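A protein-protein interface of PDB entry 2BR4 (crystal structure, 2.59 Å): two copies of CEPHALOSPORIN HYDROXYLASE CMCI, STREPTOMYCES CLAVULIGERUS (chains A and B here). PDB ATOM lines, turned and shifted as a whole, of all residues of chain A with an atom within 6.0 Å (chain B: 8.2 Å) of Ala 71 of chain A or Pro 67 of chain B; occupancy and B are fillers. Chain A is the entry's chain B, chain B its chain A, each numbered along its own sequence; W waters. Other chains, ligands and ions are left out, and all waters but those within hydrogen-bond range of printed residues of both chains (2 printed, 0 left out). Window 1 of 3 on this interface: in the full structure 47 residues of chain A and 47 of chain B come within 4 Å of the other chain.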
ATOM      1  N   ASP A  66      16.189   3.293 -18.417  1.00  0.00           N
ATOM      2  CA  ASP A  66      17.376   3.995 -18.868  1.00  0.00           C
ATOM      3  C   ASP A  66      17.031   5.444 -19.251  1.00  0.00           C
ATOM      4  O   ASP A  66      15.859   5.799 -19.268  1.00  0.00           O
ATOM      5  CB  ASP A  66      18.147   3.171 -19.918  1.00  0.00           C
ATOM      6  CG  ASP A  66      17.407   2.996 -21.189  1.00  0.00           C
ATOM      7  OD1 ASP A  66      16.704   3.947 -21.595  1.00  0.00           O
ATOM      8  OD2 ASP A  66      17.497   1.939 -21.860  1.00  0.00           O
ATOM      9  N   PRO A  67      18.039   6.297 -19.452  1.00  0.00           N
ATOM     10  CA  PRO A  67      17.812   7.743 -19.632  1.00  0.00           C
ATOM     11  C   PRO A  67      16.766   8.144 -20.675  1.00  0.00           C
ATOM     12  O   PRO A  67      15.978   9.056 -20.413  1.00  0.00           O
ATOM     13  CB  PRO A  67      19.194   8.259 -20.042  1.00  0.00           C
ATOM     14  CG  PRO A  67      20.127   7.339 -19.386  1.00  0.00           C
ATOM     15  CD  PRO A  67      19.479   5.982 -19.467  1.00  0.00           C
ATOM     16  N   ASP A  68      16.745   7.487 -21.831  1.00  0.00           N
ATOM     17  CA  ASP A  68      15.766   7.864 -22.846  1.00  0.00           C
ATOM     18  C   ASP A  68      14.333   7.509 -22.386  1.00  0.00           C
ATOM     19  O   ASP A  68      13.375   8.192 -22.730  1.00  0.00           O
ATOM     20  CB  ASP A  68      16.114   7.305 -24.250  1.00  0.00           C
ATOM     21  CG  ASP A  68      15.955   5.795 -24.368  1.00  0.00           C
ATOM     22  OD1 ASP A  68      15.551   5.151 -23.388  1.00  0.00           O
ATOM     23  OD2 ASP A  68      16.214   5.158 -25.421  1.00  0.00           O
ATOM     24  N   THR A  69      14.205   6.483 -21.552  1.00  0.00           N
ATOM     25  CA  THR A  69      12.919   6.116 -20.960  1.00  0.00           C
ATOM     26  C   THR A  69      12.477   7.162 -19.927  1.00  0.00           C
ATOM     27  O   THR A  69      11.318   7.577 -19.893  1.00  0.00           O
ATOM     28  CB  THR A  69      13.030   4.714 -20.320  1.00  0.00           C
ATOM     29  OG1 THR A  69      13.353   3.746 -21.331  1.00  0.00           O
ATOM     30  CG2 THR A  69      11.702   4.240 -19.772  1.00  0.00           C
ATOM     31  N   GLN A  70      13.416   7.590 -19.093  1.00  0.00           N
ATOM     32  CA  GLN A  70      13.146   8.620 -18.095  1.00  0.00           C
ATOM     33  C   GLN A  70      12.601   9.889 -18.750  1.00  0.00           C
ATOM     34  O   GLN A  70      11.671  10.500 -18.224  1.00  0.00           O
ATOM     35  CB  GLN A  70      14.408   8.933 -17.287  1.00  0.00           C
ATOM     36  CG  GLN A  70      14.814   7.816 -16.339  1.00  0.00           C
ATOM     37  CD  GLN A  70      16.180   8.036 -15.730  1.00  0.00           C
ATOM     38  OE1 GLN A  70      16.427   9.094 -15.142  1.00  0.00           O
ATOM     39  NE2 GLN A  70      17.070   7.045 -15.851  1.00  0.00           N
ATOM     40  N   ALA A  71      13.164  10.261 -19.900  1.00  0.00           N
ATOM     41  CA  ALA A  71      12.737  11.461 -20.630  1.00  0.00           C
ATOM     42  C   ALA A  71      11.297  11.373 -21.142  1.00  0.00           C
ATOM     43  O   ALA A  71      10.550  12.366 -21.081  1.00  0.00           O
ATOM     44  CB  ALA A  71      13.676  11.740 -21.793  1.00  0.00           C
ATOM     45  N   VAL A  72      10.922  10.203 -21.659  1.00  0.00           N
ATOM     46  CA  VAL A  72       9.552   9.952 -22.107  1.00  0.00           C
ATOM     47  C   VAL A  72       8.593  10.019 -20.932  1.00  0.00           C
ATOM     48  O   VAL A  72       7.536  10.630 -21.046  1.00  0.00           O
ATOM     49  CB  VAL A  72       9.380   8.581 -22.800  1.00  0.00           C
ATOM     50  CG1 VAL A  72       7.905   8.320 -23.106  1.00  0.00           C
ATOM     51  CG2 VAL A  72      10.220   8.500 -24.085  1.00  0.00           C
ATOM     52  N   TYR A  73       8.960   9.407 -19.808  1.00  0.00           N
ATOM     53  CA  TYR A  73       8.125   9.454 -18.609  1.00  0.00           C
ATOM     54  C   TYR A  73       8.038  10.854 -17.988  1.00  0.00           C
ATOM     55  O   TYR A  73       7.020  11.194 -17.409  1.00  0.00           O
ATOM     56  CB  TYR A  73       8.567   8.422 -17.552  1.00  0.00           C
ATOM     57  CG  TYR A  73       8.017   7.032 -17.808  1.00  0.00           C
ATOM     58  CD1 TYR A  73       8.870   5.952 -18.032  1.00  0.00           C
ATOM     59  CD2 TYR A  73       6.641   6.801 -17.847  1.00  0.00           C
ATOM     60  CE1 TYR A  73       8.373   4.680 -18.273  1.00  0.00           C
ATOM     61  CE2 TYR A  73       6.128   5.527 -18.091  1.00  0.00           C
ATOM     62  CZ  TYR A  73       7.004   4.463 -18.301  1.00  0.00           C
ATOM     63  OH  TYR A  73       6.514   3.195 -18.546  1.00  0.00           O
ATOM     64  N   HIS A  74       9.081  11.669 -18.104  1.00  0.00           N
ATOM     65  CA  HIS A  74       8.998  13.029 -17.583  1.00  0.00           C
ATOM     66  C   HIS A  74       7.951  13.798 -18.370  1.00  0.00           C
ATOM     67  O   HIS A  74       7.051  14.386 -17.783  1.00  0.00           O
ATOM     68  CB  HIS A  74      10.315  13.788 -17.668  1.00  0.00           C
ATOM     69  CG  HIS A  74      10.143  15.253 -17.426  1.00  0.00           C
ATOM     70  ND1 HIS A  74      10.213  15.809 -16.167  1.00  0.00           N
ATOM     71  CD2 HIS A  74       9.797  16.260 -18.263  1.00  0.00           C
ATOM     72  CE1 HIS A  74       9.961  17.102 -16.246  1.00  0.00           C
ATOM     73  NE2 HIS A  74       9.702  17.402 -17.506  1.00  0.00           N
ATOM     74  N   ASP A  75       8.076  13.769 -19.698  1.00  0.00           N
ATOM     75  CA  ASP A  75       7.140  14.451 -20.605  1.00  0.00           C
ATOM     76  C   ASP A  75       5.704  13.973 -20.417  1.00  0.00           C
ATOM     77  O   ASP A  75       4.771  14.767 -20.464  1.00  0.00           O
ATOM     78  CB  ASP A  75       7.528  14.234 -22.073  1.00  0.00           C
ATOM     79  CG  ASP A  75       8.902  14.767 -22.403  1.00  0.00           C
ATOM     80  OD1 ASP A  75       9.458  15.527 -21.584  1.00  0.00           O
ATOM     81  OD2 ASP A  75       9.506  14.459 -23.459  1.00  0.00           O
ATOM     82  N   MET A  76       5.548  12.668 -20.219  1.00  0.00           N
ATOM     83  CA  MET A  76       4.240  12.062 -20.033  1.00  0.00           C
ATOM     84  C   MET A  76       3.633  12.543 -18.720  1.00  0.00           C
ATOM     85  O   MET A  76       2.459  12.879 -18.674  1.00  0.00           O
ATOM     86  CB  MET A  76       4.333  10.527 -20.062  1.00  0.00           C
ATOM     87  CG  MET A  76       2.972   9.834 -20.113  1.00  0.00           C
ATOM     88  SD  MET A  76       3.002   8.012 -20.050  1.00  0.00           S
ATOM     89  CE  MET A  76       4.106   7.640 -21.448  1.00  0.00           C
ATOM     90  N   TRP A  98      11.272   7.161  -7.897  1.00  0.00           N
ATOM     91  CA  TRP A  98      11.519   8.133  -8.940  1.00  0.00           C
ATOM     92  C   TRP A  98      10.200   8.762  -9.395  1.00  0.00           C
ATOM     93  O   TRP A  98      10.086   9.980  -9.469  1.00  0.00           O
ATOM     94  CB  TRP A  98      12.233   7.447 -10.105  1.00  0.00           C
ATOM     95  CG  TRP A  98      12.572   8.344 -11.256  1.00  0.00           C
ATOM     96  CD1 TRP A  98      13.545   9.289 -11.297  1.00  0.00           C
ATOM     97  CD2 TRP A  98      11.946   8.363 -12.537  1.00  0.00           C
ATOM     98  NE1 TRP A  98      13.563   9.906 -12.524  1.00  0.00           N
ATOM     99  CE2 TRP A  98      12.585   9.356 -13.305  1.00  0.00           C
ATOM    100  CE3 TRP A  98      10.900   7.638 -13.119  1.00  0.00           C
ATOM    101  CZ2 TRP A  98      12.217   9.647 -14.606  1.00  0.00           C
ATOM    102  CZ3 TRP A  98      10.537   7.928 -14.419  1.00  0.00           C
ATOM    103  CH2 TRP A  98      11.198   8.925 -15.148  1.00  0.00           C
ATOM    104  N   TYR B  24       9.781  26.435 -24.319  1.00  0.00           N
ATOM    105  CA  TYR B  24       9.448  25.055 -24.666  1.00  0.00           C
ATOM    106  C   TYR B  24       8.071  24.953 -25.298  1.00  0.00           C
ATOM    107  O   TYR B  24       7.117  25.555 -24.826  1.00  0.00           O
ATOM    108  CB  TYR B  24       9.486  24.132 -23.443  1.00  0.00           C
ATOM    109  CG  TYR B  24       8.958  22.734 -23.729  1.00  0.00           C
ATOM    110  CD1 TYR B  24       9.697  21.837 -24.505  1.00  0.00           C
ATOM    111  CD2 TYR B  24       7.716  22.314 -23.243  1.00  0.00           C
ATOM    112  CE1 TYR B  24       9.223  20.561 -24.782  1.00  0.00           C
ATOM    113  CE2 TYR B  24       7.233  21.030 -23.508  1.00  0.00           C
ATOM    114  CZ  TYR B  24       7.993  20.161 -24.280  1.00  0.00           C
ATOM    115  OH  TYR B  24       7.536  18.891 -24.558  1.00  0.00           O
ATOM    116  N   TYR B  50       9.344  13.632 -35.445  1.00  0.00           N
ATOM    117  CA  TYR B  50       9.598  15.068 -35.341  1.00  0.00           C
ATOM    118  C   TYR B  50      11.084  15.426 -35.299  1.00  0.00           C
ATOM    119  O   TYR B  50      11.906  14.686 -34.759  1.00  0.00           O
ATOM    120  CB  TYR B  50       8.875  15.672 -34.130  1.00  0.00           C
ATOM    121  CG  TYR B  50       9.156  14.999 -32.801  1.00  0.00           C
ATOM    122  CD1 TYR B  50      10.260  15.355 -32.033  1.00  0.00           C
ATOM    123  CD2 TYR B  50       8.294  14.024 -32.296  1.00  0.00           C
ATOM    124  CE1 TYR B  50      10.512  14.752 -30.805  1.00  0.00           C
ATOM    125  CE2 TYR B  50       8.538  13.411 -31.060  1.00  0.00           C
ATOM    126  CZ  TYR B  50       9.643  13.784 -30.327  1.00  0.00           C
ATOM    127  OH  TYR B  50       9.881  13.180 -29.121  1.00  0.00           O
ATOM    128  N   SER B  54      16.515  19.647 -29.799  1.00  0.00           N
ATOM    129  CA  SER B  54      16.869  18.989 -28.554  1.00  0.00           C
ATOM    130  C   SER B  54      15.566  18.970 -27.778  1.00  0.00           C
ATOM    131  O   SER B  54      15.271  19.909 -27.041  1.00  0.00           O
ATOM    132  CB  SER B  54      17.953  19.782 -27.810  1.00  0.00           C
ATOM    133  OG  SER B  54      17.892  19.574 -26.401  1.00  0.00           O
ATOM    134  N   PRO B  55      14.765  17.928 -27.989  1.00  0.00           N
ATOM    135  CA  PRO B  55      13.387  17.892 -27.492  1.00  0.00           C
ATOM    136  C   PRO B  55      13.314  17.390 -26.052  1.00  0.00           C
ATOM    137  O   PRO B  55      12.599  16.434 -25.751  1.00  0.00           O
ATOM    138  CB  PRO B  55      12.717  16.916 -28.460  1.00  0.00           C
ATOM    139  CG  PRO B  55      13.800  15.936 -28.781  1.00  0.00           C
ATOM    140  CD  PRO B  55      15.104  16.695 -28.725  1.00  0.00           C
ATOM    141  N   TYR B  56      14.079  18.024 -25.174  1.00  0.00           N
ATOM    142  CA  TYR B  56      14.139  17.623 -23.781  1.00  0.00           C
ATOM    143  C   TYR B  56      13.772  18.818 -22.932  1.00  0.00           C
ATOM    144  O   TYR B  56      14.023  19.952 -23.303  1.00  0.00           O
ATOM    145  CB  TYR B  56      15.526  17.097 -23.426  1.00  0.00           C
ATOM    146  CG  TYR B  56      15.970  15.963 -24.321  1.00  0.00           C
ATOM    147  CD1 TYR B  56      17.034  16.116 -25.208  1.00  0.00           C
ATOM    148  CD2 TYR B  56      15.311  14.742 -24.300  1.00  0.00           C
ATOM    149  CE1 TYR B  56      17.439  15.060 -26.041  1.00  0.00           C
ATOM    150  CE2 TYR B  56      15.701  13.692 -25.129  1.00  0.00           C
ATOM    151  CZ  TYR B  56      16.764  13.856 -25.990  1.00  0.00           C
ATOM    152  OH  TYR B  56      17.139  12.810 -26.797  1.00  0.00           O
ATOM    153  N   GLN B  57      13.143  18.546 -21.802  1.00  0.00           N
ATOM    154  CA  GLN B  57      12.611  19.589 -20.962  1.00  0.00           C
ATOM    155  C   GLN B  57      12.562  19.128 -19.526  1.00  0.00           C
ATOM    156  O   GLN B  57      12.474  17.944 -19.251  1.00  0.00           O
ATOM    157  CB  GLN B  57      11.196  19.981 -21.419  1.00  0.00           C
ATOM    158  CG  GLN B  57      10.222  18.790 -21.575  1.00  0.00           C
ATOM    159  CD  GLN B  57       8.885  18.990 -20.871  1.00  0.00           C
ATOM    160  OE1 GLN B  57       8.763  19.831 -19.981  1.00  0.00           O
ATOM    161  NE2 GLN B  57       7.878  18.212 -21.272  1.00  0.00           N
ATOM    162  N   MET B  63      15.586  21.961 -22.085  1.00  0.00           N
ATOM    163  CA  MET B  63      16.834  21.462 -21.523  1.00  0.00           C
ATOM    164  C   MET B  63      17.749  21.118 -22.680  1.00  0.00           C
ATOM    165  O   MET B  63      17.374  20.326 -23.555  1.00  0.00           O
ATOM    166  CB  MET B  63      16.590  20.180 -20.725  1.00  0.00           C
ATOM    167  CG  MET B  63      15.981  20.385 -19.358  1.00  0.00           C
ATOM    168  SD  MET B  63      17.214  20.607 -18.095  1.00  0.00           S
ATOM    169  CE  MET B  63      17.778  18.928 -17.908  1.00  0.00           C
ATOM    170  N   LEU B  64      18.942  21.704 -22.694  1.00  0.00           N
ATOM    171  CA  LEU B  64      19.932  21.358 -23.712  1.00  0.00           C
ATOM    172  C   LEU B  64      20.801  20.188 -23.276  1.00  0.00           C
ATOM    173  O   LEU B  64      21.512  19.609 -24.086  1.00  0.00           O
ATOM    174  CB  LEU B  64      20.791  22.562 -24.074  1.00  0.00           C
ATOM    175  CG  LEU B  64      19.949  23.718 -24.621  1.00  0.00           C
ATOM    176  CD1 LEU B  64      20.696  24.995 -24.454  1.00  0.00           C
ATOM    177  CD2 LEU B  64      19.598  23.518 -26.083  1.00  0.00           C
ATOM    178  N   LYS B  65      20.742  19.829 -22.004  1.00  0.00           N
ATOM    179  CA  LYS B  65      21.416  18.629 -21.538  1.00  0.00           C
ATOM    180  C   LYS B  65      20.550  17.419 -21.890  1.00  0.00           C
ATOM    181  O   LYS B  65      19.398  17.318 -21.469  1.00  0.00           O
ATOM    182  CB  LYS B  65      21.689  18.725 -20.041  1.00  0.00           C
ATOM    183  CG  LYS B  65      22.555  19.934 -19.702  1.00  0.00           C
ATOM    184  CD  LYS B  65      23.111  19.910 -18.302  1.00  0.00           C
ATOM    185  CE  LYS B  65      23.842  21.226 -17.949  1.00  0.00           C
ATOM    186  NZ  LYS B  65      24.330  22.029 -19.122  1.00  0.00           N
ATOM    187  N   ASP B  66      21.082  16.523 -22.709  1.00  0.00           N
ATOM    188  CA  ASP B  66      20.310  15.367 -23.139  1.00  0.00           C
ATOM    189  C   ASP B  66      20.383  14.270 -22.055  1.00  0.00           C
ATOM    190  O   ASP B  66      21.209  14.369 -21.154  1.00  0.00           O
ATOM    191  CB  ASP B  66      20.743  14.919 -24.549  1.00  0.00           C
ATOM    192  CG  ASP B  66      22.101  14.249 -24.582  1.00  0.00           C
ATOM    193  OD1 ASP B  66      22.576  13.750 -23.531  1.00  0.00           O
ATOM    194  OD2 ASP B  66      22.758  14.154 -25.646  1.00  0.00           O
ATOM    195  N   PRO B  67      19.499  13.266 -22.117  1.00  0.00           N
ATOM    196  CA  PRO B  67      19.329  12.297 -21.022  1.00  0.00           C
ATOM    197  C   PRO B  67      20.585  11.608 -20.511  1.00  0.00           C
ATOM    198  O   PRO B  67      20.654  11.328 -19.315  1.00  0.00           O
ATOM    199  CB  PRO B  67      18.377  11.271 -21.627  1.00  0.00           C
ATOM    200  CG  PRO B  67      17.559  12.073 -22.561  1.00  0.00           C
ATOM    201  CD  PRO B  67      18.544  12.996 -23.210  1.00  0.00           C
ATOM    202  N   ASP B  68      21.550  11.330 -21.377  1.00  0.00           N
ATOM    203  CA  ASP B  68      22.783  10.676 -20.934  1.00  0.00           C
ATOM    204  C   ASP B  68      23.620  11.612 -20.079  1.00  0.00           C
ATOM    205  O   ASP B  68      24.189  11.205 -19.071  1.00  0.00           O
ATOM    206  CB  ASP B  68      23.577  10.180 -22.137  1.00  0.00           C
ATOM    207  CG  ASP B  68      22.805   9.152 -22.930  1.00  0.00           C
ATOM    208  OD1 ASP B  68      22.639   9.337 -24.162  1.00  0.00           O
ATOM    209  OD2 ASP B  68      22.281   8.150 -22.384  1.00  0.00           O
ATOM    210  N   THR B  69      23.690  12.868 -20.501  1.00  0.00           N
ATOM    211  CA  THR B  69      24.307  13.916 -19.705  1.00  0.00           C
ATOM    212  C   THR B  69      23.600  14.072 -18.359  1.00  0.00           C
ATOM    213  O   THR B  69      24.250  14.283 -17.350  1.00  0.00           O
ATOM    214  CB  THR B  69      24.288  15.241 -20.476  1.00  0.00           C
ATOM    215  OG1 THR B  69      24.957  15.073 -21.726  1.00  0.00           O
ATOM    216  CG2 THR B  69      25.111  16.300 -19.772  1.00  0.00           C
ATOM    217  N   GLN B  70      22.280  13.937 -18.351  1.00  0.00           N
ATOM    218  CA  GLN B  70      21.493  14.081 -17.133  1.00  0.00           C
ATOM    219  C   GLN B  70      21.802  12.981 -16.120  1.00  0.00           C
ATOM    220  O   GLN B  70      21.820  13.235 -14.923  1.00  0.00           O
ATOM    221  CB  GLN B  70      19.991  14.098 -17.449  1.00  0.00           C
ATOM    222  CG  GLN B  70      19.521  15.333 -18.238  1.00  0.00           C
ATOM    223  CD  GLN B  70      18.028  15.288 -18.576  1.00  0.00           C
ATOM    224  OE1 GLN B  70      17.214  14.870 -17.751  1.00  0.00           O
ATOM    225  NE2 GLN B  70      17.674  15.721 -19.771  1.00  0.00           N
ATOM    226  N   ALA B  71      22.045  11.768 -16.599  1.00  0.00           N
ATOM    227  CA  ALA B  71      22.341  10.647 -15.721  1.00  0.00           C
ATOM    228  C   ALA B  71      23.744  10.762 -15.093  1.00  0.00           C
ATOM    229  O   ALA B  71      23.966  10.345 -13.954  1.00  0.00           O
ATOM    230  CB  ALA B  71      22.208   9.332 -16.482  1.00  0.00           C
ATOM    231  N   VAL B  72      24.689  11.312 -15.848  1.00  0.00           N
ATOM    232  CA  VAL B  72      26.021  11.549 -15.325  1.00  0.00           C
ATOM    233  C   VAL B  72      25.938  12.583 -14.198  1.00  0.00           C
ATOM    234  O   VAL B  72      26.510  12.381 -13.140  1.00  0.00           O
ATOM    235  CB  VAL B  72      26.997  11.989 -16.440  1.00  0.00           C
ATOM    236  CG1 VAL B  72      28.324  12.448 -15.869  1.00  0.00           C
ATOM    237  CG2 VAL B  72      27.220  10.853 -17.411  1.00  0.00           C
ATOM    238  N   TYR B  73      25.213  13.675 -14.415  1.00  0.00           N
ATOM    239  CA  TYR B  73      25.081  14.713 -13.383  1.00  0.00           C
ATOM    240  C   TYR B  73      24.320  14.168 -12.173  1.00  0.00           C
ATOM    241  O   TYR B  73      24.666  14.469 -11.038  1.00  0.00           O
ATOM    242  CB  TYR B  73      24.422  15.989 -13.942  1.00  0.00           C
ATOM    243  CG  TYR B  73      25.400  16.927 -14.651  1.00  0.00           C
ATOM    244  CD1 TYR B  73      25.289  17.183 -16.010  1.00  0.00           C
ATOM    245  CD2 TYR B  73      26.439  17.544 -13.955  1.00  0.00           C
ATOM    246  CE1 TYR B  73      26.179  18.025 -16.655  1.00  0.00           C
ATOM    247  CE2 TYR B  73      27.337  18.389 -14.588  1.00  0.00           C
ATOM    248  CZ  TYR B  73      27.206  18.620 -15.940  1.00  0.00           C
ATOM    249  OH  TYR B  73      28.083  19.455 -16.586  1.00  0.00           O
ATOM    250  N   HIS B  74      23.315  13.325 -12.402  1.00  0.00           N
ATOM    251  CA  HIS B  74      22.657  12.654 -11.284  1.00  0.00           C
ATOM    252  C   HIS B  74      23.691  11.964 -10.390  1.00  0.00           C
ATOM    253  O   HIS B  74      23.729  12.178  -9.178  1.00  0.00           O
ATOM    254  CB  HIS B  74      21.660  11.586 -11.727  1.00  0.00           C
ATOM    255  CG  HIS B  74      21.086  10.833 -10.568  1.00  0.00           C
ATOM    256  ND1 HIS B  74      21.798   9.873  -9.880  1.00  0.00           N
ATOM    257  CD2 HIS B  74      19.913  10.977  -9.906  1.00  0.00           C
ATOM    258  CE1 HIS B  74      21.069   9.426  -8.873  1.00  0.00           C
ATOM    259  NE2 HIS B  74      19.924  10.086  -8.862  1.00  0.00           N
ATOM    260  N   TRP B  98      16.700  22.521 -13.062  1.00  0.00           N
ATOM    261  CA  TRP B  98      16.918  21.088 -12.959  1.00  0.00           C
ATOM    262  C   TRP B  98      17.910  20.781 -11.828  1.00  0.00           C
ATOM    263  O   TRP B  98      17.651  19.922 -10.984  1.00  0.00           O
ATOM    264  CB  TRP B  98      17.437  20.546 -14.297  1.00  0.00           C
ATOM    265  CG  TRP B  98      17.654  19.076 -14.293  1.00  0.00           C
ATOM    266  CD1 TRP B  98      16.695  18.119 -14.280  1.00  0.00           C
ATOM    267  CD2 TRP B  98      18.908  18.385 -14.275  1.00  0.00           C
ATOM    268  NE1 TRP B  98      17.267  16.869 -14.267  1.00  0.00           N
ATOM    269  CE2 TRP B  98      18.627  17.006 -14.270  1.00  0.00           C
ATOM    270  CE3 TRP B  98      20.244  18.791 -14.285  1.00  0.00           C
ATOM    271  CZ2 TRP B  98      19.626  16.037 -14.255  1.00  0.00           C
ATOM    272  CZ3 TRP B  98      21.239  17.828 -14.277  1.00  0.00           C
ATOM    273  CH2 TRP B  98      20.922  16.464 -14.259  1.00  0.00           C
ATOM    274  N   ALA B 220      30.989   8.861 -20.333  1.00  0.00           N
ATOM    275  CA  ALA B 220      29.629   8.370 -20.093  1.00  0.00           C
ATOM    276  C   ALA B 220      28.551   9.127 -20.866  1.00  0.00           C
ATOM    277  O   ALA B 220      27.426   8.649 -20.986  1.00  0.00           O
ATOM    278  CB  ALA B 220      29.323   8.397 -18.615  1.00  0.00           C
ATOM    279  N   SER B 221      28.881  10.307 -21.369  1.00  0.00           N
ATOM    280  CA  SER B 221      27.971  11.046 -22.242  1.00  0.00           C
ATOM    281  C   SER B 221      28.739  11.712 -23.363  1.00  0.00           C
ATOM    282  O   SER B 221      29.923  11.995 -23.231  1.00  0.00           O
ATOM    283  CB  SER B 221      27.181  12.086 -21.445  1.00  0.00           C
ATOM    284  OG  SER B 221      27.756  13.368 -21.534  1.00  0.00           O
ATOM    285  N   GLN B 223      28.063  14.718 -24.688  1.00  0.00           N
ATOM    286  CA  GLN B 223      28.201  16.149 -24.397  1.00  0.00           C
ATOM    287  C   GLN B 223      29.358  16.419 -23.426  1.00  0.00           C
ATOM    288  O   GLN B 223      30.043  17.425 -23.553  1.00  0.00           O
ATOM    289  CB  GLN B 223      26.892  16.746 -23.842  1.00  0.00           C
ATOM    290  CG  GLN B 223      25.770  16.952 -24.883  1.00  0.00           C
ATOM    291  CD  GLN B 223      24.452  17.427 -24.254  1.00  0.00           C
ATOM    292  OE1 GLN B 223      24.012  16.880 -23.246  1.00  0.00           O
ATOM    293  NE2 GLN B 223      23.832  18.438 -24.846  1.00  0.00           N
HETATM  294  O   HOH W   1      12.034  14.244 -24.258  1.00  0.00           O
HETATM  295  O   HOH W   2      12.366  15.486 -21.520  1.00  0.00           O
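The side-chain carboxylate (OD1) of Asp 75 of chain A is in hydrogen-bond range of the side-chain amide nitrogen (NE2) of Gln 57 of chain B, 3.1 Å away.
NE2 of His 74 of chain A sits close to O of Gln 57 of chain B, 3.3 Å away.
OH of Tyr 24 of chain B sits at hydrogen-bond distance from NE2 of Gln 57 of chain B (3.4 Å).
OD1 of Asp 66 of chain B lies close to N of Asp 68 of chain B (3.4 Å).
Among the printed residues, pairs that only touch across the chains: Pro 67 of chain A with Pro 67 of chain B, Pro 67 of chain A with Asp 68 of chain B and Ala 71 of chain A with Pro 67 of chain B.
Printed residues of chain B within 4 Å of Ala 71 of chain A: Pro 67.
Of the printed residues of chain B, His 74 of chain A touches Gln 57.
Of the printed residues of chain A, Gln 57 of chain B touches His 74 (3.3 Å) and Asp 75 (3.1 Å).
Printed residues of chain A within 4 Å of Pro 67 of chain B: Pro 67 and Ala 71.
Printed residues of chain A within 4 Å of Asp 68 of chain B: Pro 67 (3.8 Å).
Of the 12 printed residues of chain A, 4 touch a printed residue of chain B.
Hydrophobic or aromatic side chains of chain B that line the printed part of chain A: Pro 67.
Among the printed residues, 5 pairs touch across the chains.
Among the printed residues, no Asp or Glu carboxylate lies within 4 Å of a Lys or Arg side-chain nitrogen of the other chain.
Pro 67 of chain B touches its own counterpart, Pro 67 of chain A.
Pro 67 of chain A touches Asp 68 of chain B, but with the chains exchanged Asp 68 of chain A does not touch Pro 67 of chain B (4.1 Å).
Ala 71 of chain A touches Pro 67 of chain B, but with the chains exchanged Pro 67 of chain A does not touch Ala 71 of chain B (4.1 Å).
10 positions are printed for both chains.
Of the 5 pairs that touch across the chains among the printed residues, 1 has its exchanged pair printed and touching as well.
Water W1 bridges the side-chain carboxylate of Asp 75 of chain A (2.7 Å) and the backbone carbonyl oxygen of Pro 55 of chain B (2.7 Å).
Water W2 bridges OD1 of Asp 75 of chain A (2.9 Å) and N of Gln 57 of chain B (3.2 Å).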
